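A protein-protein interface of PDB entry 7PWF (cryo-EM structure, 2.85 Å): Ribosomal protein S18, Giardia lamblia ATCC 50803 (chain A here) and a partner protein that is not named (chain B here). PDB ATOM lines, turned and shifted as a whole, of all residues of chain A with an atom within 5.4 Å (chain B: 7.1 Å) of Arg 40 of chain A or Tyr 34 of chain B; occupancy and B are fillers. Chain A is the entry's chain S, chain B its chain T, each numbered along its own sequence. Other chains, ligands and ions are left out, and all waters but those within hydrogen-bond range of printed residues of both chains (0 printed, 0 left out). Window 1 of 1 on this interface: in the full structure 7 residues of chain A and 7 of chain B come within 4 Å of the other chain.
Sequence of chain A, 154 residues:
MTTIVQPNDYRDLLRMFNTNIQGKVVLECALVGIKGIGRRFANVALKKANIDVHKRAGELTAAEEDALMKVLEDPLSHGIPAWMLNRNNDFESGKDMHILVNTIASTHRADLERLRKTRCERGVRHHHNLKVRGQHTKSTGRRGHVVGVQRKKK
Of the 11 printed residues of chain B, 6 touch a printed residue of chain A.
Of the 14 printed residues of chain A, 6 touch a printed residue of chain B.
Hydrophobic or aromatic side chains of chain A that line the printed part of chain B: Val 44, Pro 81, Trp 83 and Met 84.
Among the printed residues, 10 pairs touch across the chains.
Among the printed residues, no Asp or Glu carboxylate lies within 4 Å of a Lys or Arg side-chain nitrogen of the other chain.
The backbone carbonyl oxygen (O) of Arg 39 of chain A lies within hydrogen-bond range of the side-chain amide nitrogen (ND2) of Asn 43 of chain A (2.5 Å).
O of Arg 40 of chain A lies close to OD1 of Asn 43 of chain A (2.8 Å).
Of the printed residues of chain B, Arg 40 of chain A touches Tyr 34 (3.7 Å), Val 35 (3.8 Å), Lys 36 (3.99 Å), Gln 42 (3.8 Å) and Ala 44 (3.2 Å).
Of the printed residues of chain B, Val 44 of chain A touches Tyr 34.
Of the printed residues of chain A, Val 35 of chain B touches Arg 40 (3.8 Å).
Ala 45 of chain A touches none of the printed residues of chain B.
Asn 43 of chain A touches none of the printed residues of chain B.
The nearest printed residue of chain A that does not touch Tyr 43 of chain B is Arg 40 of chain A (4.2 Å).
Among the printed residues, merely in contact across the chains: Arg 39 of chain A with Tyr 43 of chain B (3.3 Å), Arg 40 of chain A with Tyr 34 of chain B (3.7 Å), Arg 40 of chain A with Val 35 of chain B (3.8 Å), Arg 40 of chain A with Lys 36 of chain B (3.99 Å), Arg 40 of chain A with Gln 42 of chain B (3.8 Å), Arg 40 of chain A with Ala 44 of chain B (3.2 Å), Val 44 of chain A with Tyr 34 of chain B (3.5 Å), Pro 81 of chain A with Tyr 34 of chain B (3.5 Å), Trp 83 of chain A with Tyr 34 of chain B (3.2 Å) and Met 84 of chain A with Tyr 34 of chain B (3.4 Å).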
ATOM      1  N   GLY A  38      34.881   5.248 -15.991  1.00  0.00           N
ATOM      2  CA  GLY A  38      33.924   4.185 -16.221  1.00  0.00           C
ATOM      3  C   GLY A  38      33.377   4.318 -17.624  1.00  0.00           C
ATOM      4  O   GLY A  38      33.847   5.171 -18.377  1.00  0.00           O
ATOM      5  N   ARG A  39      32.407   3.492 -18.009  1.00  0.00           N
ATOM      6  CA  ARG A  39      31.795   3.715 -19.312  1.00  0.00           C
ATOM      7  C   ARG A  39      30.844   4.906 -19.256  1.00  0.00           C
ATOM      8  O   ARG A  39      30.654   5.600 -20.258  1.00  0.00           O
ATOM      9  CB  ARG A  39      31.063   2.462 -19.787  1.00  0.00           C
ATOM     10  CG  ARG A  39      30.508   2.598 -21.191  1.00  0.00           C
ATOM     11  CD  ARG A  39      29.238   1.802 -21.393  1.00  0.00           C
ATOM     12  NE  ARG A  39      28.960   1.514 -22.790  1.00  0.00           N
ATOM     13  CZ  ARG A  39      29.655   0.655 -23.521  1.00  0.00           C
ATOM     14  NH1 ARG A  39      30.636  -0.046 -22.970  1.00  0.00           N
ATOM     15  NH2 ARG A  39      29.337   0.461 -24.792  1.00  0.00           N
ATOM     16  N   ARG A  40      30.262   5.166 -18.084  1.00  0.00           N
ATOM     17  CA  ARG A  40      29.427   6.346 -17.887  1.00  0.00           C
ATOM     18  C   ARG A  40      30.247   7.624 -18.044  1.00  0.00           C
ATOM     19  O   ARG A  40      29.929   8.493 -18.866  1.00  0.00           O
ATOM     20  CB  ARG A  40      28.783   6.284 -16.498  1.00  0.00           C
ATOM     21  CG  ARG A  40      27.621   5.303 -16.384  1.00  0.00           C
ATOM     22  CD  ARG A  40      26.468   5.599 -17.343  1.00  0.00           C
ATOM     23  NE  ARG A  40      25.591   6.669 -16.874  1.00  0.00           N
ATOM     24  CZ  ARG A  40      25.060   7.598 -17.662  1.00  0.00           C
ATOM     25  NH1 ARG A  40      24.259   8.523 -17.156  1.00  0.00           N
ATOM     26  NH2 ARG A  40      25.323   7.597 -18.959  1.00  0.00           N
ATOM     27  N   PHE A  41      31.311   7.753 -17.251  1.00  0.00           N
ATOM     28  CA  PHE A  41      32.143   8.947 -17.312  1.00  0.00           C
ATOM     29  C   PHE A  41      32.784   9.111 -18.684  1.00  0.00           C
ATOM     30  O   PHE A  41      32.946  10.235 -19.165  1.00  0.00           O
ATOM     31  CB  PHE A  41      33.204   8.894 -16.217  1.00  0.00           C
ATOM     32  CG  PHE A  41      33.900  10.200 -15.978  1.00  0.00           C
ATOM     33  CD1 PHE A  41      33.233  11.259 -15.390  1.00  0.00           C
ATOM     34  CD2 PHE A  41      35.225  10.367 -16.336  1.00  0.00           C
ATOM     35  CE1 PHE A  41      33.869  12.458 -15.172  1.00  0.00           C
ATOM     36  CE2 PHE A  41      35.868  11.564 -16.119  1.00  0.00           C
ATOM     37  CZ  PHE A  41      35.188  12.609 -15.535  1.00  0.00           C
ATOM     38  N   ALA A  42      33.129   8.006 -19.345  1.00  0.00           N
ATOM     39  CA  ALA A  42      33.700   8.117 -20.683  1.00  0.00           C
ATOM     40  C   ALA A  42      32.665   8.598 -21.689  1.00  0.00           C
ATOM     41  O   ALA A  42      32.941   9.500 -22.491  1.00  0.00           O
ATOM     42  CB  ALA A  42      34.292   6.778 -21.119  1.00  0.00           C
ATOM     43  N   ASN A  43      31.465   8.013 -21.673  1.00  0.00           N
ATOM     44  CA  ASN A  43      30.478   8.504 -22.619  1.00  0.00           C
ATOM     45  C   ASN A  43      29.971   9.888 -22.251  1.00  0.00           C
ATOM     46  O   ASN A  43      29.224  10.468 -23.034  1.00  0.00           O
ATOM     47  CB  ASN A  43      29.297   7.527 -22.773  1.00  0.00           C
ATOM     48  CG  ASN A  43      28.489   7.344 -21.494  1.00  0.00           C
ATOM     49  OD1 ASN A  43      27.978   8.299 -20.914  1.00  0.00           O
ATOM     50  ND2 ASN A  43      28.344   6.092 -21.071  1.00  0.00           N
ATOM     51  N   VAL A  44      30.326  10.429 -21.084  1.00  0.00           N
ATOM     52  CA  VAL A  44      30.031  11.838 -20.830  1.00  0.00           C
ATOM     53  C   VAL A  44      31.244  12.731 -21.067  1.00  0.00           C
ATOM     54  O   VAL A  44      31.111  13.961 -21.061  1.00  0.00           O
ATOM     55  CB  VAL A  44      29.472  12.064 -19.408  1.00  0.00           C
ATOM     56  CG1 VAL A  44      30.565  11.975 -18.365  1.00  0.00           C
ATOM     57  CG2 VAL A  44      28.730  13.388 -19.313  1.00  0.00           C
ATOM     58  N   ALA A  45      32.423  12.153 -21.284  1.00  0.00           N
ATOM     59  CA  ALA A  45      33.597  12.964 -21.580  1.00  0.00           C
ATOM     60  C   ALA A  45      33.910  13.059 -23.066  1.00  0.00           C
ATOM     61  O   ALA A  45      34.526  14.044 -23.488  1.00  0.00           O
ATOM     62  CB  ALA A  45      34.824  12.418 -20.844  1.00  0.00           C
ATOM     63  N   LYS A  48      30.823  15.313 -24.833  1.00  0.00           N
ATOM     64  CA  LYS A  48      30.990  16.669 -24.327  1.00  0.00           C
ATOM     65  C   LYS A  48      32.141  17.408 -25.008  1.00  0.00           C
ATOM     66  O   LYS A  48      32.198  18.641 -24.942  1.00  0.00           O
ATOM     67  CB  LYS A  48      31.202  16.616 -22.811  1.00  0.00           C
ATOM     68  CG  LYS A  48      31.290  17.962 -22.132  1.00  0.00           C
ATOM     69  CD  LYS A  48      30.002  18.749 -22.284  1.00  0.00           C
ATOM     70  CE  LYS A  48      28.823  18.033 -21.653  1.00  0.00           C
ATOM     71  NZ  LYS A  48      27.891  18.998 -21.008  1.00  0.00           N
ATOM     72  N   GLY A  79      30.394  21.639 -18.250  1.00  0.00           N
ATOM     73  CA  GLY A  79      29.005  21.351 -17.956  1.00  0.00           C
ATOM     74  C   GLY A  79      28.702  19.963 -17.433  1.00  0.00           C
ATOM     75  O   GLY A  79      27.536  19.677 -17.148  1.00  0.00           O
ATOM     76  N   ILE A  80      29.703  19.098 -17.306  1.00  0.00           N
ATOM     77  CA  ILE A  80      29.506  17.813 -16.623  1.00  0.00           C
ATOM     78  C   ILE A  80      29.104  18.079 -15.177  1.00  0.00           C
ATOM     79  O   ILE A  80      29.770  18.878 -14.491  1.00  0.00           O
ATOM     80  CB  ILE A  80      30.789  16.966 -16.696  1.00  0.00           C
ATOM     81  CG1 ILE A  80      31.410  17.059 -18.092  1.00  0.00           C
ATOM     82  CG2 ILE A  80      30.509  15.520 -16.336  1.00  0.00           C
ATOM     83  CD1 ILE A  80      32.839  16.581 -18.157  1.00  0.00           C
ATOM     84  N   PRO A  81      28.047  17.455 -14.664  1.00  0.00           N
ATOM     85  CA  PRO A  81      27.483  17.867 -13.373  1.00  0.00           C
ATOM     86  C   PRO A  81      28.219  17.270 -12.180  1.00  0.00           C
ATOM     87  O   PRO A  81      29.072  16.391 -12.301  1.00  0.00           O
ATOM     88  CB  PRO A  81      26.043  17.338 -13.432  1.00  0.00           C
ATOM     89  CG  PRO A  81      25.822  16.912 -14.851  1.00  0.00           C
ATOM     90  CD  PRO A  81      27.163  16.511 -15.359  1.00  0.00           C
ATOM     91  N   TRP A  83      26.674  15.564  -9.652  1.00  0.00           N
ATOM     92  CA  TRP A  83      26.164  14.236  -9.321  1.00  0.00           C
ATOM     93  C   TRP A  83      26.818  13.144 -10.161  1.00  0.00           C
ATOM     94  O   TRP A  83      26.830  11.977  -9.755  1.00  0.00           O
ATOM     95  CB  TRP A  83      24.649  14.216  -9.474  1.00  0.00           C
ATOM     96  CG  TRP A  83      24.178  14.302 -10.883  1.00  0.00           C
ATOM     97  CD1 TRP A  83      23.864  15.433 -11.562  1.00  0.00           C
ATOM     98  CD2 TRP A  83      23.934  13.213 -11.781  1.00  0.00           C
ATOM     99  NE1 TRP A  83      23.454  15.125 -12.832  1.00  0.00           N
ATOM    100  CE2 TRP A  83      23.487  13.766 -12.991  1.00  0.00           C
ATOM    101  CE3 TRP A  83      24.061  11.827 -11.680  1.00  0.00           C
ATOM    102  CZ2 TRP A  83      23.161  12.983 -14.094  1.00  0.00           C
ATOM    103  CZ3 TRP A  83      23.744  11.054 -12.775  1.00  0.00           C
ATOM    104  CH2 TRP A  83      23.292  11.631 -13.965  1.00  0.00           C
ATOM    105  N   MET A  84      27.378  13.498 -11.319  1.00  0.00           N
ATOM    106  CA  MET A  84      28.150  12.566 -12.133  1.00  0.00           C
ATOM    107  C   MET A  84      29.642  12.606 -11.822  1.00  0.00           C
ATOM    108  O   MET A  84      30.470  12.343 -12.703  1.00  0.00           O
ATOM    109  CB  MET A  84      27.914  12.839 -13.619  1.00  0.00           C
ATOM    110  CG  MET A  84      28.240  11.657 -14.504  1.00  0.00           C
ATOM    111  SD  MET A  84      27.357  11.677 -16.055  1.00  0.00           S
ATOM    112  CE  MET A  84      26.106  10.470 -15.678  1.00  0.00           C
ATOM    113  N   ALA B  30      18.793  20.249 -23.403  1.00  0.00           N
ATOM    114  CA  ALA B  30      20.201  20.023 -23.108  1.00  0.00           C
ATOM    115  C   ALA B  30      20.454  18.911 -22.098  1.00  0.00           C
ATOM    116  O   ALA B  30      21.464  18.210 -22.213  1.00  0.00           O
ATOM    117  CB  ALA B  30      20.844  21.315 -22.592  1.00  0.00           C
ATOM    118  N   PHE B  31      19.565  18.720 -21.123  1.00  0.00           N
ATOM    119  CA  PHE B  31      19.726  17.651 -20.142  1.00  0.00           C
ATOM    120  C   PHE B  31      19.796  16.262 -20.773  1.00  0.00           C
ATOM    121  O   PHE B  31      20.043  15.289 -20.055  1.00  0.00           O
ATOM    122  CB  PHE B  31      18.585  17.700 -19.124  1.00  0.00           C
ATOM    123  N   THR B  32      19.574  16.152 -22.086  1.00  0.00           N
ATOM    124  CA  THR B  32      19.601  14.863 -22.768  1.00  0.00           C
ATOM    125  C   THR B  32      20.912  14.114 -22.570  1.00  0.00           C
ATOM    126  O   THR B  32      20.927  12.879 -22.581  1.00  0.00           O
ATOM    127  CB  THR B  32      19.340  15.060 -24.260  1.00  0.00           C
ATOM    128  OG1 THR B  32      19.342  13.791 -24.921  1.00  0.00           O
ATOM    129  CG2 THR B  32      20.392  15.960 -24.882  1.00  0.00           C
ATOM    130  N   ASP B  33      22.024  14.826 -22.427  1.00  0.00           N
ATOM    131  CA  ASP B  33      23.271  14.134 -22.159  1.00  0.00           C
ATOM    132  C   ASP B  33      23.289  13.631 -20.720  1.00  0.00           C
ATOM    133  O   ASP B  33      22.511  14.070 -19.873  1.00  0.00           O
ATOM    134  CB  ASP B  33      24.464  15.050 -22.421  1.00  0.00           C
ATOM    135  CG  ASP B  33      24.476  15.592 -23.838  1.00  0.00           C
ATOM    136  OD1 ASP B  33      24.571  14.784 -24.788  1.00  0.00           O
ATOM    137  OD2 ASP B  33      24.387  16.826 -24.001  1.00  0.00           O
ATOM    138  N   TYR B  34      24.169  12.668 -20.465  1.00  0.00           N
ATOM    139  CA  TYR B  34      24.449  12.152 -19.126  1.00  0.00           C
ATOM    140  C   TYR B  34      23.177  11.811 -18.349  1.00  0.00           C
ATOM    141  O   TYR B  34      23.048  12.105 -17.159  1.00  0.00           O
ATOM    142  CB  TYR B  34      25.337  13.129 -18.341  1.00  0.00           C
ATOM    143  CG  TYR B  34      24.863  14.568 -18.239  1.00  0.00           C
ATOM    144  CD1 TYR B  34      23.794  14.923 -17.424  1.00  0.00           C
ATOM    145  CD2 TYR B  34      25.523  15.580 -18.920  1.00  0.00           C
ATOM    146  CE1 TYR B  34      23.376  16.231 -17.326  1.00  0.00           C
ATOM    147  CE2 TYR B  34      25.112  16.891 -18.824  1.00  0.00           C
ATOM    148  CZ  TYR B  34      24.041  17.212 -18.022  1.00  0.00           C
ATOM    149  OH  TYR B  34      23.628  18.521 -17.920  1.00  0.00           O
ATOM    150  N   VAL B  35      22.235  11.156 -19.023  1.00  0.00           N
ATOM    151  CA  VAL B  35      21.006  10.711 -18.375  1.00  0.00           C
ATOM    152  C   VAL B  35      20.687   9.298 -18.845  1.00  0.00           C
ATOM    153  O   VAL B  35      20.787   8.993 -20.040  1.00  0.00           O
ATOM    154  CB  VAL B  35      19.823  11.670 -18.644  1.00  0.00           C
ATOM    155  CG1 VAL B  35      19.441  11.692 -20.111  1.00  0.00           C
ATOM    156  CG2 VAL B  35      18.620  11.312 -17.776  1.00  0.00           C
ATOM    157  N   LYS B  36      20.338   8.427 -17.904  1.00  0.00           N
ATOM    158  CA  LYS B  36      19.783   7.121 -18.220  1.00  0.00           C
ATOM    159  C   LYS B  36      18.282   7.251 -18.408  1.00  0.00           C
ATOM    160  O   LYS B  36      17.616   7.963 -17.654  1.00  0.00           O
ATOM    161  CB  LYS B  36      20.074   6.113 -17.105  1.00  0.00           C
ATOM    162  CG  LYS B  36      21.483   5.604 -17.071  1.00  0.00           C
ATOM    163  CD  LYS B  36      21.666   4.573 -15.973  1.00  0.00           C
ATOM    164  CE  LYS B  36      21.334   5.136 -14.603  1.00  0.00           C
ATOM    165  NZ  LYS B  36      20.657   4.121 -13.740  1.00  0.00           N
ATOM    166  N   GLN B  42      21.695   0.466 -17.146  1.00  0.00           N
ATOM    167  CA  GLN B  42      23.006   0.715 -16.578  1.00  0.00           C
ATOM    168  C   GLN B  42      23.860   1.645 -17.426  1.00  0.00           C
ATOM    169  O   GLN B  42      24.884   2.124 -16.935  1.00  0.00           O
ATOM    170  CB  GLN B  42      23.746  -0.606 -16.309  1.00  0.00           C
ATOM    171  CG  GLN B  42      23.663  -1.681 -17.377  1.00  0.00           C
ATOM    172  CD  GLN B  42      24.561  -2.874 -17.048  1.00  0.00           C
ATOM    173  OE1 GLN B  42      24.619  -3.845 -17.797  1.00  0.00           O
ATOM    174  NE2 GLN B  42      25.278  -2.789 -15.945  1.00  0.00           N
ATOM    175  N   TYR B  43      23.448   1.949 -18.656  1.00  0.00           N
ATOM    176  CA  TYR B  43      24.157   2.902 -19.498  1.00  0.00           C
ATOM    177  C   TYR B  43      23.148   3.796 -20.204  1.00  0.00           C
ATOM    178  O   TYR B  43      21.950   3.516 -20.230  1.00  0.00           O
ATOM    179  CB  TYR B  43      25.044   2.208 -20.535  1.00  0.00           C
ATOM    180  CG  TYR B  43      26.041   1.248 -19.945  1.00  0.00           C
ATOM    181  CD1 TYR B  43      26.991   1.676 -19.029  1.00  0.00           C
ATOM    182  CD2 TYR B  43      26.069  -0.079 -20.345  1.00  0.00           C
ATOM    183  CE1 TYR B  43      27.911   0.796 -18.490  1.00  0.00           C
ATOM    184  CE2 TYR B  43      26.992  -0.961 -19.824  1.00  0.00           C
ATOM    185  CZ  TYR B  43      27.913  -0.518 -18.901  1.00  0.00           C
ATOM    186  OH  TYR B  43      28.830  -1.400 -18.380  1.00  0.00           O
ATOM    187  N   ALA B  44      23.649   4.883 -20.781  1.00  0.00           N
ATOM    188  CA  ALA B  44      22.837   5.803 -21.559  1.00  0.00           C
ATOM    189  C   ALA B  44      22.631   5.269 -22.970  1.00  0.00           C
ATOM    190  O   ALA B  44      23.420   4.453 -23.452  1.00  0.00           O
ATOM    191  CB  ALA B  44      23.500   7.174 -21.616  1.00  0.00           C
ATOM    192  N   PRO B  45      21.565   5.696 -23.651  1.00  0.00           N
ATOM    193  CA  PRO B  45      21.358   5.243 -25.029  1.00  0.00           C
ATOM    194  C   PRO B  45      22.483   5.727 -25.927  1.00  0.00           C
ATOM    195  O   PRO B  45      23.064   6.792 -25.717  1.00  0.00           O
ATOM    196  CB  PRO B  45      20.015   5.871 -25.419  1.00  0.00           C
ATOM    197  CG  PRO B  45      19.785   6.945 -24.443  1.00  0.00           C
ATOM    198  CD  PRO B  45      20.453   6.537 -23.181  1.00  0.00           C
